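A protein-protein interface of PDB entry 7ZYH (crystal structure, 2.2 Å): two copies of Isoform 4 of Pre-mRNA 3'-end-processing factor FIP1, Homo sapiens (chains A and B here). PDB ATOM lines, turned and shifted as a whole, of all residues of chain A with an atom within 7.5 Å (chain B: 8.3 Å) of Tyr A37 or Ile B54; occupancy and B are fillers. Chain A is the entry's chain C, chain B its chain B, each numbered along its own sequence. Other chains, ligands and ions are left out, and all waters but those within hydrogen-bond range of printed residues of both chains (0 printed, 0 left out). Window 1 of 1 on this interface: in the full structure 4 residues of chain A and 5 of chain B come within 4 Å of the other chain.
NH2 of Arg B55 sits close to N of Gly A38, at 3.4 Å.
OE1 of Gln B51 lies within hydrogen-bond range of NH1 of Arg B55 (2.6 Å). The side-chain hydroxyl (OH) of Tyr B47 sits at hydrogen-bond distance from the side-chain amide nitrogen (NE2) of Gln B51 (2.8 Å).
Among the printed residues, merely in contact across the chains: Tyr A37 with Lys B50 (3.0 Å), Tyr A37 with Gln B51 (3.2 Å), Tyr A37 with Ile B54 (3.1 Å), Tyr A37 with Arg B55 (3.5 Å) and Phe A39 with Ile B54 (3.9 Å).
Of chain B, only Lys B50, Gln B51, Ile B54 and Arg B55 come within 4 Å of Tyr A37. Ile B54 touches just these residues of chain A: Tyr A37 (3.1 Å) and Phe A39 (3.9 Å). No residue of chain B comes within 4 Å of Asn A36. Printed residues of chain B within 4 Å of Gly A38: Arg B55 (3.4 Å). Of the printed residues of chain A, Lys B50 touches Tyr A37. Printed residues of chain B within 4 Å of Phe A39: Ile B54 (3.9 Å). Of the printed residues of chain A, Arg B55 touches Tyr A37 (3.5 Å) and Gly A38 (3.4 Å). Printed residues of chain A within 4 Å of Gln B51: Tyr A37 (3.2 Å). The nearest residue of chain B that does not touch Tyr A37 is Tyr B47 (4.5 Å). The nearest residue of chain A that does not touch Ile B54 is Tyr A47 (4.2 Å).
Of the 13 printed residues of chain B, 4 touch a printed residue of chain A. Hydrophobic or aromatic side chains of chain B that line the printed part of chain A: Ile B54. Along chain B the printed residues that touch a printed residue of chain A span positions 50 to 55. Among the printed residues, no Asp or Glu carboxylate lies within 4 Å of a Lys or Arg side-chain nitrogen of the other chain.
2 positions are printed for both chains. Of the 6 pairs that touch across the chains among the printed residues, none has its exchanged pair printed and touching as well.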
ATOM      1  N   SER A  32      -6.585  30.955  12.987  1.00  0.00           N
ATOM      2  CA  SER A  32      -5.289  31.478  13.391  1.00  0.00           C
ATOM      3  C   SER A  32      -5.445  32.542  14.460  1.00  0.00           C
ATOM      4  O   SER A  32      -4.520  32.752  15.247  1.00  0.00           O
ATOM      5  CB  SER A  32      -4.551  32.067  12.194  1.00  0.00           C
ATOM      6  OG  SER A  32      -4.257  31.064  11.244  1.00  0.00           O
ATOM      7  N   PHE A  35      -6.139  29.711  17.544  1.00  0.00           N
ATOM      8  CA  PHE A  35      -5.180  28.641  17.798  1.00  0.00           C
ATOM      9  C   PHE A  35      -3.847  29.041  17.175  1.00  0.00           C
ATOM     10  O   PHE A  35      -3.780  29.369  15.985  1.00  0.00           O
ATOM     11  CB  PHE A  35      -5.617  27.267  17.239  1.00  0.00           C
ATOM     12  CG  PHE A  35      -6.753  26.628  18.001  1.00  0.00           C
ATOM     13  CD1 PHE A  35      -6.542  26.094  19.258  1.00  0.00           C
ATOM     14  CD2 PHE A  35      -8.026  26.554  17.453  1.00  0.00           C
ATOM     15  CE1 PHE A  35      -7.582  25.531  19.963  1.00  0.00           C
ATOM     16  CE2 PHE A  35      -9.061  25.976  18.148  1.00  0.00           C
ATOM     17  CZ  PHE A  35      -8.840  25.462  19.401  1.00  0.00           C
ATOM     18  N   ASN A  36      -2.788  28.988  17.969  1.00  0.00           N
ATOM     19  CA  ASN A  36      -1.437  29.217  17.500  1.00  0.00           C
ATOM     20  C   ASN A  36      -0.825  27.895  17.051  1.00  0.00           C
ATOM     21  O   ASN A  36      -1.353  26.814  17.302  1.00  0.00           O
ATOM     22  CB  ASN A  36      -0.666  29.913  18.620  1.00  0.00           C
ATOM     23  CG  ASN A  36       0.532  30.680  18.126  1.00  0.00           C
ATOM     24  OD1 ASN A  36       0.864  30.645  16.939  1.00  0.00           O
ATOM     25  ND2 ASN A  36       1.134  31.454  19.016  1.00  0.00           N
ATOM     26  N   TYR A  37       0.288  28.000  16.344  1.00  0.00           N
ATOM     27  CA  TYR A  37       1.021  26.842  15.849  1.00  0.00           C
ATOM     28  C   TYR A  37       0.180  25.969  14.927  1.00  0.00           C
ATOM     29  O   TYR A  37       0.495  24.793  14.737  1.00  0.00           O
ATOM     30  CB  TYR A  37       1.543  25.979  17.003  1.00  0.00           C
ATOM     31  CG  TYR A  37       2.141  26.763  18.146  1.00  0.00           C
ATOM     32  CD1 TYR A  37       3.400  27.364  18.031  1.00  0.00           C
ATOM     33  CD2 TYR A  37       1.431  26.918  19.337  1.00  0.00           C
ATOM     34  CE1 TYR A  37       3.937  28.097  19.070  1.00  0.00           C
ATOM     35  CE2 TYR A  37       1.951  27.631  20.381  1.00  0.00           C
ATOM     36  CZ  TYR A  37       3.206  28.232  20.239  1.00  0.00           C
ATOM     37  OH  TYR A  37       3.711  28.939  21.293  1.00  0.00           O
ATOM     38  N   GLY A  38      -0.887  26.513  14.353  1.00  0.00           N
ATOM     39  CA  GLY A  38      -1.767  25.714  13.527  1.00  0.00           C
ATOM     40  C   GLY A  38      -2.557  24.670  14.281  1.00  0.00           C
ATOM     41  O   GLY A  38      -2.928  23.646  13.699  1.00  0.00           O
ATOM     42  N   PHE A  39      -2.826  24.903  15.563  1.00  0.00           N
ATOM     43  CA  PHE A  39      -3.638  23.979  16.338  1.00  0.00           C
ATOM     44  C   PHE A  39      -5.064  23.936  15.794  1.00  0.00           C
ATOM     45  O   PHE A  39      -5.513  24.838  15.083  1.00  0.00           O
ATOM     46  CB  PHE A  39      -3.687  24.396  17.805  1.00  0.00           C
ATOM     47  CG  PHE A  39      -2.532  23.887  18.634  1.00  0.00           C
ATOM     48  CD1 PHE A  39      -2.247  22.535  18.718  1.00  0.00           C
ATOM     49  CD2 PHE A  39      -1.742  24.770  19.342  1.00  0.00           C
ATOM     50  CE1 PHE A  39      -1.193  22.082  19.486  1.00  0.00           C
ATOM     51  CE2 PHE A  39      -0.690  24.320  20.106  1.00  0.00           C
ATOM     52  CZ  PHE A  39      -0.416  22.975  20.178  1.00  0.00           C
ATOM     53  N   ASN A  40      -5.770  22.859  16.129  1.00  0.00           N
ATOM     54  CA  ASN A  40      -7.208  22.750  15.939  1.00  0.00           C
ATOM     55  C   ASN A  40      -7.855  22.484  17.293  1.00  0.00           C
ATOM     56  O   ASN A  40      -7.177  22.152  18.271  1.00  0.00           O
ATOM     57  CB  ASN A  40      -7.556  21.625  14.965  1.00  0.00           C
ATOM     58  CG  ASN A  40      -8.491  22.076  13.869  1.00  0.00           C
ATOM     59  OD1 ASN A  40      -9.183  23.086  13.994  1.00  0.00           O
ATOM     60  ND2 ASN A  40      -8.523  21.318  12.781  1.00  0.00           N
ATOM     61  N   THR A  43      -6.775  19.165  17.992  1.00  0.00           N
ATOM     62  CA  THR A  43      -5.330  19.098  18.177  1.00  0.00           C
ATOM     63  C   THR A  43      -4.902  19.818  19.449  1.00  0.00           C
ATOM     64  O   THR A  43      -3.961  19.390  20.131  1.00  0.00           O
ATOM     65  CB  THR A  43      -4.619  19.704  16.967  1.00  0.00           C
ATOM     66  OG1 THR A  43      -5.166  19.146  15.768  1.00  0.00           O
ATOM     67  CG2 THR A  43      -3.123  19.387  17.033  1.00  0.00           C
ATOM     68  N   TRP A  44      -5.565  20.923  19.777  1.00  0.00           N
ATOM     69  CA  TRP A  44      -5.238  21.634  21.006  1.00  0.00           C
ATOM     70  C   TRP A  44      -5.564  20.785  22.225  1.00  0.00           C
ATOM     71  O   TRP A  44      -4.743  20.657  23.138  1.00  0.00           O
ATOM     72  CB  TRP A  44      -5.982  22.968  21.048  1.00  0.00           C
ATOM     73  CG  TRP A  44      -5.844  23.710  22.333  1.00  0.00           C
ATOM     74  CD1 TRP A  44      -6.835  24.033  23.209  1.00  0.00           C
ATOM     75  CD2 TRP A  44      -4.628  24.217  22.898  1.00  0.00           C
ATOM     76  NE1 TRP A  44      -6.313  24.718  24.279  1.00  0.00           N
ATOM     77  CE2 TRP A  44      -4.958  24.841  24.111  1.00  0.00           C
ATOM     78  CE3 TRP A  44      -3.291  24.199  22.493  1.00  0.00           C
ATOM     79  CZ2 TRP A  44      -4.002  25.439  24.925  1.00  0.00           C
ATOM     80  CZ3 TRP A  44      -2.352  24.787  23.301  1.00  0.00           C
ATOM     81  CH2 TRP A  44      -2.708  25.403  24.501  1.00  0.00           C
ATOM     82  N   TYR A  47      -2.981  18.090  22.366  1.00  0.00           N
ATOM     83  CA  TYR A  47      -1.804  18.732  22.937  1.00  0.00           C
ATOM     84  C   TYR A  47      -1.974  18.920  24.432  1.00  0.00           C
ATOM     85  O   TYR A  47      -1.077  18.601  25.218  1.00  0.00           O
ATOM     86  CB  TYR A  47      -1.584  20.071  22.235  1.00  0.00           C
ATOM     87  CG  TYR A  47      -0.455  20.920  22.772  1.00  0.00           C
ATOM     88  CD1 TYR A  47       0.857  20.704  22.375  1.00  0.00           C
ATOM     89  CD2 TYR A  47      -0.708  21.954  23.662  1.00  0.00           C
ATOM     90  CE1 TYR A  47       1.885  21.490  22.862  1.00  0.00           C
ATOM     91  CE2 TYR A  47       0.311  22.741  24.151  1.00  0.00           C
ATOM     92  CZ  TYR A  47       1.605  22.508  23.749  1.00  0.00           C
ATOM     93  OH  TYR A  47       2.619  23.303  24.237  1.00  0.00           O
ATOM     94  N   GLN A  51       0.253  17.198  27.287  1.00  0.00           N
ATOM     95  CA  GLN A  51       1.041  17.967  28.241  1.00  0.00           C
ATOM     96  C   GLN A  51       0.716  17.592  29.682  1.00  0.00           C
ATOM     97  O   GLN A  51       1.608  17.545  30.534  1.00  0.00           O
ATOM     98  CB  GLN A  51       0.791  19.456  28.032  1.00  0.00           C
ATOM     99  CG  GLN A  51       1.321  20.075  26.743  1.00  0.00           C
ATOM    100  CD  GLN A  51       2.834  20.054  26.698  1.00  0.00           C
ATOM    101  OE1 GLN A  51       3.497  20.262  27.717  1.00  0.00           O
ATOM    102  NE2 GLN A  51       3.391  19.842  25.509  1.00  0.00           N
ATOM    103  N   ALA B  46      14.035  30.988  21.440  1.00  0.00           N
ATOM    104  CA  ALA B  46      13.210  29.961  22.067  1.00  0.00           C
ATOM    105  C   ALA B  46      11.827  29.914  21.425  1.00  0.00           C
ATOM    106  O   ALA B  46      11.262  28.833  21.216  1.00  0.00           O
ATOM    107  CB  ALA B  46      13.088  30.226  23.569  1.00  0.00           C
ATOM    108  N   TYR B  47      11.277  31.080  21.086  1.00  0.00           N
ATOM    109  CA  TYR B  47       9.955  31.131  20.475  1.00  0.00           C
ATOM    110  C   TYR B  47       9.980  30.484  19.097  1.00  0.00           C
ATOM    111  O   TYR B  47       9.034  29.790  18.713  1.00  0.00           O
ATOM    112  CB  TYR B  47       9.480  32.584  20.407  1.00  0.00           C
ATOM    113  CG  TYR B  47       8.178  32.822  19.671  1.00  0.00           C
ATOM    114  CD1 TYR B  47       6.979  32.317  20.159  1.00  0.00           C
ATOM    115  CD2 TYR B  47       8.141  33.575  18.508  1.00  0.00           C
ATOM    116  CE1 TYR B  47       5.788  32.544  19.503  1.00  0.00           C
ATOM    117  CE2 TYR B  47       6.953  33.805  17.841  1.00  0.00           C
ATOM    118  CZ  TYR B  47       5.782  33.307  18.355  1.00  0.00           C
ATOM    119  OH  TYR B  47       4.598  33.523  17.694  1.00  0.00           O
ATOM    120  N   CYS B  48      11.068  30.678  18.351  1.00  0.00           N
ATOM    121  CA  CYS B  48      11.187  30.039  17.049  1.00  0.00           C
ATOM    122  C   CYS B  48      11.351  28.531  17.185  1.00  0.00           C
ATOM    123  O   CYS B  48      10.737  27.777  16.429  1.00  0.00           O
ATOM    124  CB  CYS B  48      12.357  30.640  16.276  1.00  0.00           C
ATOM    125  SG  CYS B  48      12.180  32.366  15.861  1.00  0.00           S
ATOM    126  N   GLU B  49      12.142  28.061  18.155  1.00  0.00           N
ATOM    127  CA  GLU B  49      12.254  26.617  18.358  1.00  0.00           C
ATOM    128  C   GLU B  49      10.893  26.010  18.671  1.00  0.00           C
ATOM    129  O   GLU B  49      10.514  24.973  18.114  1.00  0.00           O
ATOM    130  CB  GLU B  49      13.259  26.290  19.466  1.00  0.00           C
ATOM    131  CG  GLU B  49      14.452  25.470  18.962  1.00  0.00           C
ATOM    132  CD  GLU B  49      14.038  24.187  18.240  1.00  0.00           C
ATOM    133  OE1 GLU B  49      13.009  23.598  18.628  1.00  0.00           O
ATOM    134  OE2 GLU B  49      14.727  23.790  17.275  1.00  0.00           O
ATOM    135  N   LYS B  50      10.147  26.629  19.585  1.00  0.00           N
ATOM    136  CA  LYS B  50       8.810  26.134  19.889  1.00  0.00           C
ATOM    137  C   LYS B  50       7.963  26.064  18.628  1.00  0.00           C
ATOM    138  O   LYS B  50       7.265  25.073  18.384  1.00  0.00           O
ATOM    139  CB  LYS B  50       8.126  27.031  20.922  1.00  0.00           C
ATOM    140  CG  LYS B  50       6.700  26.585  21.199  1.00  0.00           C
ATOM    141  CD  LYS B  50       6.060  27.366  22.331  1.00  0.00           C
ATOM    142  CE  LYS B  50       5.756  26.371  23.475  1.00  0.00           C
ATOM    143  NZ  LYS B  50       4.766  26.926  24.422  1.00  0.00           N
ATOM    144  N   GLN B  51       7.981  27.123  17.826  1.00  0.00           N
ATOM    145  CA  GLN B  51       7.260  27.089  16.561  1.00  0.00           C
ATOM    146  C   GLN B  51       7.683  25.879  15.747  1.00  0.00           C
ATOM    147  O   GLN B  51       6.847  25.127  15.237  1.00  0.00           O
ATOM    148  CB  GLN B  51       7.520  28.354  15.761  1.00  0.00           C
ATOM    149  CG  GLN B  51       6.992  29.580  16.427  1.00  0.00           C
ATOM    150  CD  GLN B  51       5.490  29.769  16.242  1.00  0.00           C
ATOM    151  OE1 GLN B  51       4.842  28.952  15.605  1.00  0.00           O
ATOM    152  NE2 GLN B  51       4.937  30.856  16.802  1.00  0.00           N
ATOM    153  N   LYS B  52       8.995  25.659  15.640  1.00  0.00           N
ATOM    154  CA  LYS B  52       9.495  24.568  14.813  1.00  0.00           C
ATOM    155  C   LYS B  52       8.968  23.234  15.313  1.00  0.00           C
ATOM    156  O   LYS B  52       8.385  22.455  14.551  1.00  0.00           O
ATOM    157  CB  LYS B  52      11.022  24.544  14.865  1.00  0.00           C
ATOM    158  CG  LYS B  52      11.753  25.744  14.290  1.00  0.00           C
ATOM    159  CD  LYS B  52      13.258  25.495  14.428  1.00  0.00           C
ATOM    160  CE  LYS B  52      14.025  26.786  14.638  1.00  0.00           C
ATOM    161  NZ  LYS B  52      15.074  26.578  15.689  1.00  0.00           N
ATOM    162  N   ARG B  53       9.164  22.956  16.602  1.00  0.00           N
ATOM    163  CA  ARG B  53       8.730  21.680  17.157  1.00  0.00           C
ATOM    164  C   ARG B  53       7.222  21.504  17.066  1.00  0.00           C
ATOM    165  O   ARG B  53       6.735  20.471  16.597  1.00  0.00           O
ATOM    166  CB  ARG B  53       9.190  21.539  18.604  1.00  0.00           C
ATOM    167  CG  ARG B  53      10.618  21.079  18.744  1.00  0.00           C
ATOM    168  CD  ARG B  53      10.807  20.303  20.048  1.00  0.00           C
ATOM    169  NE  ARG B  53      12.199  19.912  20.229  1.00  0.00           N
ATOM    170  CZ  ARG B  53      12.924  20.188  21.302  1.00  0.00           C
ATOM    171  NH1 ARG B  53      12.394  20.789  22.355  1.00  0.00           N
ATOM    172  NH2 ARG B  53      14.210  19.844  21.323  1.00  0.00           N
ATOM    173  N   ILE B  54       6.461  22.487  17.535  1.00  0.00           N
ATOM    174  CA  ILE B  54       5.024  22.283  17.669  1.00  0.00           C
ATOM    175  C   ILE B  54       4.391  22.013  16.310  1.00  0.00           C
ATOM    176  O   ILE B  54       3.678  21.019  16.126  1.00  0.00           O
ATOM    177  CB  ILE B  54       4.374  23.491  18.360  1.00  0.00           C
ATOM    178  CG1 ILE B  54       4.673  23.484  19.858  1.00  0.00           C
ATOM    179  CG2 ILE B  54       2.879  23.455  18.161  1.00  0.00           C
ATOM    180  CD1 ILE B  54       4.145  24.697  20.597  1.00  0.00           C
ATOM    181  N   ARG B  55       4.626  22.902  15.340  1.00  0.00           N
ATOM    182  CA  ARG B  55       4.016  22.731  14.027  1.00  0.00           C
ATOM    183  C   ARG B  55       4.456  21.445  13.339  1.00  0.00           C
ATOM    184  O   ARG B  55       3.864  21.082  12.315  1.00  0.00           O
ATOM    185  CB  ARG B  55       4.335  23.937  13.134  1.00  0.00           C
ATOM    186  CG  ARG B  55       4.055  25.293  13.786  1.00  0.00           C
ATOM    187  CD  ARG B  55       4.151  26.467  12.812  1.00  0.00           C
ATOM    188  NE  ARG B  55       2.833  26.993  12.477  1.00  0.00           N
ATOM    189  CZ  ARG B  55       2.376  28.175  12.872  1.00  0.00           C
ATOM    190  NH1 ARG B  55       3.101  28.981  13.626  1.00  0.00           N
ATOM    191  NH2 ARG B  55       1.160  28.559  12.496  1.00  0.00           N
ATOM    192  N   MET B  56       5.414  20.708  13.904  1.00  0.00           N
ATOM    193  CA  MET B  56       5.911  19.488  13.269  1.00  0.00           C
ATOM    194  C   MET B  56       6.543  18.617  14.339  1.00  0.00           C
ATOM    195  O   MET B  56       7.580  18.978  14.906  1.00  0.00           O
ATOM    196  CB  MET B  56       6.946  19.784  12.185  1.00  0.00           C
ATOM    197  CG  MET B  56       6.655  20.871  11.198  1.00  0.00           C
ATOM    198  SD  MET B  56       8.188  21.194  10.288  1.00  0.00           S
ATOM    199  CE  MET B  56       7.581  22.129   8.895  1.00  0.00           C
ATOM    200  N   GLY B  57       5.936  17.463  14.590  1.00  0.00           N
ATOM    201  CA  GLY B  57       6.510  16.510  15.510  1.00  0.00           C
ATOM    202  C   GLY B  57       5.609  16.179  16.680  1.00  0.00           C
ATOM    203  O   GLY B  57       4.395  16.355  16.591  1.00  0.00           O
ATOM    204  N   LEU B  58       6.196  15.723  17.784  1.00  0.00           N
ATOM    205  CA  LEU B  58       5.440  15.393  18.990  1.00  0.00           C
ATOM    206  C   LEU B  58       4.249  14.512  18.651  1.00  0.00           C
ATOM    207  O   LEU B  58       4.170  13.371  19.099  1.00  0.00           O
ATOM    208  CB  LEU B  58       4.989  16.671  19.689  1.00  0.00           C
ATOM    209  CG  LEU B  58       3.954  16.525  20.797  1.00  0.00           C
ATOM    210  CD1 LEU B  58       4.113  17.644  21.828  1.00  0.00           C
ATOM    211  CD2 LEU B  58       2.540  16.540  20.235  1.00  0.00           C
